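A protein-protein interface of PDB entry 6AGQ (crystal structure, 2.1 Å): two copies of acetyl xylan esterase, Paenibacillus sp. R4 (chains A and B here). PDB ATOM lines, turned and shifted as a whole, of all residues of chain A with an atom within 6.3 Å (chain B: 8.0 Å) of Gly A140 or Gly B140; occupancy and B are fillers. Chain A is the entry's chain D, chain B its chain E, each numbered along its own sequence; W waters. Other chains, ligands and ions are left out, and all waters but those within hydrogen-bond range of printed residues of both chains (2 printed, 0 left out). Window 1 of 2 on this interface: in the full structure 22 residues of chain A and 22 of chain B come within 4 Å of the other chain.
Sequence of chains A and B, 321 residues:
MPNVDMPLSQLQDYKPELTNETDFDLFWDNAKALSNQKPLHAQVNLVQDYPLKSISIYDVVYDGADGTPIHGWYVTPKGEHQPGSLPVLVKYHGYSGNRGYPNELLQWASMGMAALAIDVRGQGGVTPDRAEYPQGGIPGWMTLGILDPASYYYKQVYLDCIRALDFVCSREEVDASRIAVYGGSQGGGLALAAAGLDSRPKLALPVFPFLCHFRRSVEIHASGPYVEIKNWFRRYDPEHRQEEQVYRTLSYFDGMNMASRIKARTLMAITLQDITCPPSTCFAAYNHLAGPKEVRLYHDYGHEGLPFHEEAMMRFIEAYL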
ATOM      1  N   TYR A  95      -0.287  35.201  18.046  1.00  0.00           N
ATOM      2  CA  TYR A  95       1.094  34.879  17.881  1.00  0.00           C
ATOM      3  C   TYR A  95       1.463  33.784  18.858  1.00  0.00           C
ATOM      4  O   TYR A  95       1.243  33.922  20.049  1.00  0.00           O
ATOM      5  CB  TYR A  95       1.919  36.119  18.093  1.00  0.00           C
ATOM      6  CG  TYR A  95       3.390  35.945  17.768  1.00  0.00           C
ATOM      7  CD1 TYR A  95       3.868  36.162  16.466  1.00  0.00           C
ATOM      8  CD2 TYR A  95       4.300  35.638  18.786  1.00  0.00           C
ATOM      9  CE1 TYR A  95       5.232  36.051  16.174  1.00  0.00           C
ATOM     10  CE2 TYR A  95       5.654  35.535  18.514  1.00  0.00           C
ATOM     11  CZ  TYR A  95       6.128  35.769  17.202  1.00  0.00           C
ATOM     12  OH  TYR A  95       7.481  35.622  16.906  1.00  0.00           O
ATOM     13  N   ILE A 138      16.323  35.718  15.943  1.00  0.00           N
ATOM     14  CA  ILE A 138      15.806  35.849  17.315  1.00  0.00           C
ATOM     15  C   ILE A 138      14.743  34.772  17.612  1.00  0.00           C
ATOM     16  O   ILE A 138      13.991  34.366  16.706  1.00  0.00           O
ATOM     17  CB  ILE A 138      15.205  37.255  17.473  1.00  0.00           C
ATOM     18  CG1 ILE A 138      16.224  38.347  17.122  1.00  0.00           C
ATOM     19  CG2 ILE A 138      14.661  37.542  18.878  1.00  0.00           C
ATOM     20  CD1 ILE A 138      17.647  38.132  17.667  1.00  0.00           C
ATOM     21  N   PRO A 139      14.652  34.312  18.899  1.00  0.00           N
ATOM     22  CA  PRO A 139      13.607  33.320  19.228  1.00  0.00           C
ATOM     23  C   PRO A 139      12.240  33.836  18.819  1.00  0.00           C
ATOM     24  O   PRO A 139      11.960  34.986  19.012  1.00  0.00           O
ATOM     25  CB  PRO A 139      13.719  33.133  20.762  1.00  0.00           C
ATOM     26  CG  PRO A 139      14.693  34.176  21.248  1.00  0.00           C
ATOM     27  CD  PRO A 139      15.517  34.620  20.068  1.00  0.00           C
ATOM     28  N   GLY A 140      11.436  32.977  18.190  1.00  0.00           N
ATOM     29  CA  GLY A 140      10.186  33.389  17.539  1.00  0.00           C
ATOM     30  C   GLY A 140      10.277  33.381  15.999  1.00  0.00           C
ATOM     31  O   GLY A 140      11.123  32.677  15.449  1.00  0.00           O
ATOM     32  N   TRP A 141       9.429  34.180  15.337  1.00  0.00           N
ATOM     33  CA  TRP A 141       9.244  34.090  13.886  1.00  0.00           C
ATOM     34  C   TRP A 141       9.331  35.407  13.132  1.00  0.00           C
ATOM     35  O   TRP A 141       9.548  35.388  11.913  1.00  0.00           O
ATOM     36  CB  TRP A 141       7.927  33.345  13.531  1.00  0.00           C
ATOM     37  CG  TRP A 141       7.843  31.957  14.195  1.00  0.00           C
ATOM     38  CD1 TRP A 141       8.417  30.781  13.772  1.00  0.00           C
ATOM     39  CD2 TRP A 141       7.155  31.652  15.421  1.00  0.00           C
ATOM     40  NE1 TRP A 141       8.112  29.736  14.692  1.00  0.00           N
ATOM     41  CE2 TRP A 141       7.344  30.276  15.702  1.00  0.00           C
ATOM     42  CE3 TRP A 141       6.392  32.404  16.291  1.00  0.00           C
ATOM     43  CZ2 TRP A 141       6.800  29.675  16.834  1.00  0.00           C
ATOM     44  CZ3 TRP A 141       5.867  31.808  17.413  1.00  0.00           C
ATOM     45  CH2 TRP A 141       6.077  30.459  17.683  1.00  0.00           C
ATOM     46  N   MET A 142       9.291  36.516  13.856  1.00  0.00           N
ATOM     47  CA  MET A 142       9.236  37.849  13.259  1.00  0.00           C
ATOM     48  C   MET A 142      10.527  38.249  12.543  1.00  0.00           C
ATOM     49  O   MET A 142      10.519  39.263  11.816  1.00  0.00           O
ATOM     50  CB  MET A 142       9.061  38.894  14.346  1.00  0.00           C
ATOM     51  CG  MET A 142       7.846  38.741  15.206  1.00  0.00           C
ATOM     52  SD  MET A 142       6.344  39.184  14.345  1.00  0.00           S
ATOM     53  CE  MET A 142       6.786  40.862  13.846  1.00  0.00           C
ATOM     54  N   THR A 143      11.650  37.565  12.832  1.00  0.00           N
ATOM     55  CA  THR A 143      12.900  37.987  12.237  1.00  0.00           C
ATOM     56  C   THR A 143      13.399  37.047  11.183  1.00  0.00           C
ATOM     57  O   THR A 143      14.418  37.333  10.591  1.00  0.00           O
ATOM     58  CB  THR A 143      14.018  38.273  13.284  1.00  0.00           C
ATOM     59  OG1 THR A 143      14.359  37.040  13.975  1.00  0.00           O
ATOM     60  CG2 THR A 143      13.532  39.301  14.253  1.00  0.00           C
ATOM     61  N   LEU A 144      12.693  35.964  10.903  1.00  0.00           N
ATOM     62  CA  LEU A 144      13.196  35.028   9.930  1.00  0.00           C
ATOM     63  C   LEU A 144      13.081  35.600   8.559  1.00  0.00           C
ATOM     64  O   LEU A 144      11.970  35.949   8.108  1.00  0.00           O
ATOM     65  CB  LEU A 144      12.465  33.685   9.994  1.00  0.00           C
ATOM     66  CG  LEU A 144      12.665  32.948  11.349  1.00  0.00           C
ATOM     67  CD1 LEU A 144      11.598  31.873  11.515  1.00  0.00           C
ATOM     68  CD2 LEU A 144      14.060  32.337  11.385  1.00  0.00           C
ATOM     69  N   GLU A 228      10.989  41.493  19.073  1.00  0.00           N
ATOM     70  CA  GLU A 228      11.922  40.676  18.339  1.00  0.00           C
ATOM     71  C   GLU A 228      12.681  41.507  17.308  1.00  0.00           C
ATOM     72  O   GLU A 228      13.881  41.319  17.141  1.00  0.00           O
ATOM     73  CB  GLU A 228      11.232  39.485  17.704  1.00  0.00           C
ATOM     74  CG  GLU A 228      10.761  38.404  18.697  1.00  0.00           C
ATOM     75  CD  GLU A 228       9.809  37.396  18.017  1.00  0.00           C
ATOM     76  OE1 GLU A 228      10.075  36.995  16.841  1.00  0.00           O
ATOM     77  OE2 GLU A 228       8.798  36.960  18.660  1.00  0.00           O
ATOM     78  N   TYR B  95      22.516  30.424  24.645  1.00  0.00           N
ATOM     79  CA  TYR B  95      21.261  30.276  23.939  1.00  0.00           C
ATOM     80  C   TYR B  95      20.877  31.659  23.328  1.00  0.00           C
ATOM     81  O   TYR B  95      20.867  32.694  24.024  1.00  0.00           O
ATOM     82  CB  TYR B  95      20.212  29.807  24.928  1.00  0.00           C
ATOM     83  CG  TYR B  95      18.873  29.379  24.328  1.00  0.00           C
ATOM     84  CD1 TYR B  95      18.728  28.140  23.809  1.00  0.00           C
ATOM     85  CD2 TYR B  95      17.758  30.241  24.354  1.00  0.00           C
ATOM     86  CE1 TYR B  95      17.499  27.692  23.330  1.00  0.00           C
ATOM     87  CE2 TYR B  95      16.543  29.842  23.827  1.00  0.00           C
ATOM     88  CZ  TYR B  95      16.423  28.537  23.346  1.00  0.00           C
ATOM     89  OH  TYR B  95      15.269  28.050  22.830  1.00  0.00           O
ATOM     90  N   SER B  96      20.633  31.658  22.032  1.00  0.00           N
ATOM     91  CA  SER B  96      20.209  32.796  21.221  1.00  0.00           C
ATOM     92  C   SER B  96      21.407  33.567  20.703  1.00  0.00           C
ATOM     93  O   SER B  96      21.229  34.509  19.964  1.00  0.00           O
ATOM     94  CB  SER B  96      19.220  33.763  21.954  1.00  0.00           C
ATOM     95  OG  SER B  96      19.989  34.607  22.850  1.00  0.00           O
ATOM     96  N   GLY B 122      20.598  28.351  13.455  1.00  0.00           N
ATOM     97  CA  GLY B 122      19.358  29.029  13.665  1.00  0.00           C
ATOM     98  C   GLY B 122      19.315  30.138  14.695  1.00  0.00           C
ATOM     99  O   GLY B 122      18.299  30.838  14.748  1.00  0.00           O
ATOM    100  N   GLN B 123      20.374  30.353  15.471  1.00  0.00           N
ATOM    101  CA  GLN B 123      20.294  31.293  16.601  1.00  0.00           C
ATOM    102  C   GLN B 123      20.724  32.657  16.081  1.00  0.00           C
ATOM    103  O   GLN B 123      20.606  32.876  14.881  1.00  0.00           O
ATOM    104  CB  GLN B 123      21.018  30.765  17.875  1.00  0.00           C
ATOM    105  CG  GLN B 123      20.307  29.497  18.376  1.00  0.00           C
ATOM    106  CD  GLN B 123      20.785  28.876  19.678  1.00  0.00           C
ATOM    107  OE1 GLN B 123      21.561  29.411  20.469  1.00  0.00           O
ATOM    108  NE2 GLN B 123      20.239  27.751  19.931  1.00  0.00           N
ATOM    109  N   ASP B 129      19.214  27.224   9.950  1.00  0.00           N
ATOM    110  CA  ASP B 129      18.894  25.844  10.340  1.00  0.00           C
ATOM    111  C   ASP B 129      18.219  25.201   9.158  1.00  0.00           C
ATOM    112  O   ASP B 129      17.125  25.577   8.858  1.00  0.00           O
ATOM    113  CB  ASP B 129      17.918  25.848  11.527  1.00  0.00           C
ATOM    114  CG  ASP B 129      17.613  24.439  12.087  1.00  0.00           C
ATOM    115  OD1 ASP B 129      18.222  23.463  11.596  1.00  0.00           O
ATOM    116  OD2 ASP B 129      16.710  24.300  12.995  1.00  0.00           O
ATOM    117  N   TYR B 133      11.184  19.745  10.870  1.00  0.00           N
ATOM    118  CA  TYR B 133      10.610  19.163  12.099  1.00  0.00           C
ATOM    119  C   TYR B 133       9.213  18.791  11.774  1.00  0.00           C
ATOM    120  O   TYR B 133       8.624  19.424  10.943  1.00  0.00           O
ATOM    121  CB  TYR B 133      10.633  20.218  13.220  1.00  0.00           C
ATOM    122  CG  TYR B 133      11.992  20.738  13.417  1.00  0.00           C
ATOM    123  CD1 TYR B 133      12.916  19.978  14.084  1.00  0.00           C
ATOM    124  CD2 TYR B 133      12.405  21.952  12.855  1.00  0.00           C
ATOM    125  CE1 TYR B 133      14.233  20.368  14.213  1.00  0.00           C
ATOM    126  CE2 TYR B 133      13.716  22.395  13.047  1.00  0.00           C
ATOM    127  CZ  TYR B 133      14.633  21.594  13.719  1.00  0.00           C
ATOM    128  OH  TYR B 133      15.960  21.925  13.941  1.00  0.00           O
ATOM    129  N   GLY B 136       4.983  22.150  14.771  1.00  0.00           N
ATOM    130  CA  GLY B 136       5.437  23.408  15.231  1.00  0.00           C
ATOM    131  C   GLY B 136       6.210  23.397  16.501  1.00  0.00           C
ATOM    132  O   GLY B 136       6.732  22.368  16.957  1.00  0.00           O
ATOM    133  N   GLY B 137       6.299  24.580  17.074  1.00  0.00           N
ATOM    134  CA  GLY B 137       6.656  24.718  18.471  1.00  0.00           C
ATOM    135  C   GLY B 137       6.429  26.072  19.151  1.00  0.00           C
ATOM    136  O   GLY B 137       5.787  27.011  18.638  1.00  0.00           O
ATOM    137  N   ILE B 138       6.990  26.116  20.337  1.00  0.00           N
ATOM    138  CA  ILE B 138       7.107  27.254  21.196  1.00  0.00           C
ATOM    139  C   ILE B 138       8.216  28.120  20.680  1.00  0.00           C
ATOM    140  O   ILE B 138       9.169  27.607  20.104  1.00  0.00           O
ATOM    141  CB  ILE B 138       7.436  26.796  22.605  1.00  0.00           C
ATOM    142  CG1 ILE B 138       6.340  25.809  23.075  1.00  0.00           C
ATOM    143  CG2 ILE B 138       7.547  28.002  23.548  1.00  0.00           C
ATOM    144  CD1 ILE B 138       4.925  26.380  23.068  1.00  0.00           C
ATOM    145  N   PRO B 139       8.077  29.444  20.845  1.00  0.00           N
ATOM    146  CA  PRO B 139       9.132  30.267  20.286  1.00  0.00           C
ATOM    147  C   PRO B 139      10.492  29.872  20.910  1.00  0.00           C
ATOM    148  O   PRO B 139      10.571  29.661  22.122  1.00  0.00           O
ATOM    149  CB  PRO B 139       8.736  31.700  20.732  1.00  0.00           C
ATOM    150  CG  PRO B 139       7.283  31.646  20.897  1.00  0.00           C
ATOM    151  CD  PRO B 139       6.983  30.270  21.415  1.00  0.00           C
ATOM    152  N   GLY B 140      11.534  29.818  20.073  1.00  0.00           N
ATOM    153  CA  GLY B 140      12.879  29.326  20.452  1.00  0.00           C
ATOM    154  C   GLY B 140      13.063  27.971  19.776  1.00  0.00           C
ATOM    155  O   GLY B 140      12.366  27.655  18.771  1.00  0.00           O
ATOM    156  N   TRP B 141      14.002  27.188  20.305  1.00  0.00           N
ATOM    157  CA  TRP B 141      14.483  25.982  19.627  1.00  0.00           C
ATOM    158  C   TRP B 141      14.392  24.758  20.527  1.00  0.00           C
ATOM    159  O   TRP B 141      14.450  23.680  20.030  1.00  0.00           O
ATOM    160  CB  TRP B 141      15.934  26.173  19.133  1.00  0.00           C
ATOM    161  CG  TRP B 141      16.094  27.382  18.291  1.00  0.00           C
ATOM    162  CD1 TRP B 141      15.821  27.482  16.981  1.00  0.00           C
ATOM    163  CD2 TRP B 141      16.489  28.681  18.724  1.00  0.00           C
ATOM    164  NE1 TRP B 141      16.097  28.750  16.536  1.00  0.00           N
ATOM    165  CE2 TRP B 141      16.446  29.522  17.608  1.00  0.00           C
ATOM    166  CE3 TRP B 141      16.869  29.217  19.957  1.00  0.00           C
ATOM    167  CZ2 TRP B 141      16.773  30.872  17.679  1.00  0.00           C
ATOM    168  CZ3 TRP B 141      17.168  30.535  20.035  1.00  0.00           C
ATOM    169  CH2 TRP B 141      17.132  31.359  18.898  1.00  0.00           C
ATOM    170  N   MET B 142      14.106  24.910  21.811  1.00  0.00           N
ATOM    171  CA  MET B 142      14.018  23.737  22.746  1.00  0.00           C
ATOM    172  C   MET B 142      12.949  22.753  22.444  1.00  0.00           C
ATOM    173  O   MET B 142      13.026  21.561  22.900  1.00  0.00           O
ATOM    174  CB  MET B 142      13.707  24.183  24.168  1.00  0.00           C
ATOM    175  CG  MET B 142      14.667  25.136  24.775  1.00  0.00           C
ATOM    176  SD  MET B 142      16.282  24.454  24.985  1.00  0.00           S
ATOM    177  CE  MET B 142      15.933  23.097  26.107  1.00  0.00           C
ATOM    178  N   THR B 143      11.896  23.214  21.763  1.00  0.00           N
ATOM    179  CA  THR B 143      10.772  22.352  21.501  1.00  0.00           C
ATOM    180  C   THR B 143      10.687  21.763  20.123  1.00  0.00           C
ATOM    181  O   THR B 143       9.748  20.922  19.846  1.00  0.00           O
ATOM    182  CB  THR B 143       9.444  22.988  21.910  1.00  0.00           C
ATOM    183  OG1 THR B 143       9.142  24.145  21.081  1.00  0.00           O
ATOM    184  CG2 THR B 143       9.512  23.391  23.405  1.00  0.00           C
ATOM    185  N   LEU B 144      11.643  22.114  19.260  1.00  0.00           N
ATOM    186  CA  LEU B 144      11.545  21.666  17.869  1.00  0.00           C
ATOM    187  C   LEU B 144      11.879  20.183  17.746  1.00  0.00           C
ATOM    188  O   LEU B 144      12.990  19.741  18.077  1.00  0.00           O
ATOM    189  CB  LEU B 144      12.419  22.509  16.922  1.00  0.00           C
ATOM    190  CG  LEU B 144      11.984  23.969  16.748  1.00  0.00           C
ATOM    191  CD1 LEU B 144      13.047  24.762  15.997  1.00  0.00           C
ATOM    192  CD2 LEU B 144      10.647  24.068  16.016  1.00  0.00           C
ATOM    193  N   TYR B 153      15.826  19.138  17.668  1.00  0.00           N
ATOM    194  CA  TYR B 153      16.708  20.264  17.327  1.00  0.00           C
ATOM    195  C   TYR B 153      18.172  19.979  17.714  1.00  0.00           C
ATOM    196  O   TYR B 153      19.052  20.133  16.887  1.00  0.00           O
ATOM    197  CB  TYR B 153      16.221  21.576  18.009  1.00  0.00           C
ATOM    198  CG  TYR B 153      17.167  22.759  17.932  1.00  0.00           C
ATOM    199  CD1 TYR B 153      17.289  23.477  16.746  1.00  0.00           C
ATOM    200  CD2 TYR B 153      17.917  23.160  19.031  1.00  0.00           C
ATOM    201  CE1 TYR B 153      18.158  24.536  16.632  1.00  0.00           C
ATOM    202  CE2 TYR B 153      18.786  24.256  18.931  1.00  0.00           C
ATOM    203  CZ  TYR B 153      18.934  24.908  17.724  1.00  0.00           C
ATOM    204  OH  TYR B 153      19.732  26.030  17.597  1.00  0.00           O
ATOM    205  N   PRO B 225      15.455  29.221  29.159  1.00  0.00           N
ATOM    206  CA  PRO B 225      14.821  28.382  28.138  1.00  0.00           C
ATOM    207  C   PRO B 225      14.212  27.064  28.558  1.00  0.00           C
ATOM    208  O   PRO B 225      13.373  26.549  27.793  1.00  0.00           O
ATOM    209  CB  PRO B 225      15.913  28.175  27.081  1.00  0.00           C
ATOM    210  CG  PRO B 225      17.087  28.987  27.516  1.00  0.00           C
ATOM    211  CD  PRO B 225      16.850  29.582  28.839  1.00  0.00           C
ATOM    212  N   GLU B 228      10.462  26.966  28.068  1.00  0.00           N
ATOM    213  CA  GLU B 228       9.867  26.471  26.803  1.00  0.00           C
ATOM    214  C   GLU B 228       9.239  25.070  26.927  1.00  0.00           C
ATOM    215  O   GLU B 228       8.140  24.858  26.442  1.00  0.00           O
ATOM    216  CB  GLU B 228      10.872  26.491  25.672  1.00  0.00           C
ATOM    217  CG  GLU B 228      11.246  27.885  25.241  1.00  0.00           C
ATOM    218  CD  GLU B 228      12.354  27.939  24.185  1.00  0.00           C
ATOM    219  OE1 GLU B 228      12.350  27.045  23.279  1.00  0.00           O
ATOM    220  OE2 GLU B 228      13.197  28.916  24.259  1.00  0.00           O
HETATM  221  O   HOH W   1      13.073  30.134  17.341  1.00  0.00           O
HETATM  222  O   HOH W   2      10.618  30.113  16.994  1.00  0.00           O
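OH of Tyr B95 sits at hydrogen-bond distance from N of Trp B141, at 3.0 Å.
The backbone NH (N) of Trp A141 is in hydrogen-bond range of the side-chain hydroxyl (OH) of Tyr A95 (2.9 Å).
The side-chain carboxylate of Glu A228 is in hydrogen-bond range of the backbone NH of Trp A141, 3.3 Å away.
The backbone NH of Trp B141 is in hydrogen-bond range of the side-chain carboxylate of Glu B228, at 3.4 Å.
CB of Pro A139 touches CA of Gly B140, at 3.9 Å.
CD of Pro A139 touches CH2 of Trp B141, 3.8 Å away.
CA of Gly A140 touches CB of Pro B139, at 3.9 Å.
Gly B140 touches Gly A140 (N to N, 3.7 Å).
O of Gly B137 touches CZ2 of Trp A141, 3.4 Å away.
CH2 of Trp A141 touches CG of Pro B139 (3.6 Å).
Gly A140 touches just these residues of chain B: Pro B139 and Gly B140.
Of chain A, only Pro A139 and Gly A140 come within 4 Å of Gly B140.
Of the printed residues of chain B, Pro A139 touches Gly B140 (3.9 Å) and Trp B141 (3.8 Å).
Of the printed residues of chain A, Trp B141 touches Pro A139 (3.8 Å).
Printed residues of chain A within 4 Å of Pro B139: Gly A140 and Trp A141.
Of the printed residues of chain B, Trp A141 touches Gly B137 and Pro B139.
Tyr B153 touches none of the printed residues of chain A.
Glu A228 touches none of the printed residues of chain B.
The nearest printed residue of chain A that does not touch Trp B141 is Ile A138 (4.4 Å).
Printed residues of chain A that touch a printed residue of chain B: Pro A139, Gly A140 and Trp A141.
Hydrophobic or aromatic side chains of chain A within 4 Å of the printed part of chain B: Pro A139 and Trp A141.
Printed residues of chain B that touch a printed residue of chain A: Gly B137, Pro B139, Gly B140 and Trp B141.
Hydrophobic or aromatic side chains of chain B within 4 Å of the printed part of chain A: Pro B139 and Trp B141.
Along chain B the printed residues that touch a printed residue of chain A span positions 137 to 141.
Pro A139 touches Gly B140, and with the chains exchanged Gly A140 touches Pro B139.
Pro A139 touches Trp B141, and with the chains exchanged Trp A141 touches Pro B139.
Gly A140 touches its own counterpart, Gly B140.
9 positions are printed for both chains.
Of the 6 pairs that touch across the chains among the printed residues, 5 have their exchanged pair printed and touching as well.
Water W1 lies within hydrogen-bond range of O of Gly B140, N of Gly A140 and NE1 of Trp B141.
Water W2 lies within hydrogen-bond range of O of Gly A140, N of Gly B140 and NE1 of Trp A141.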
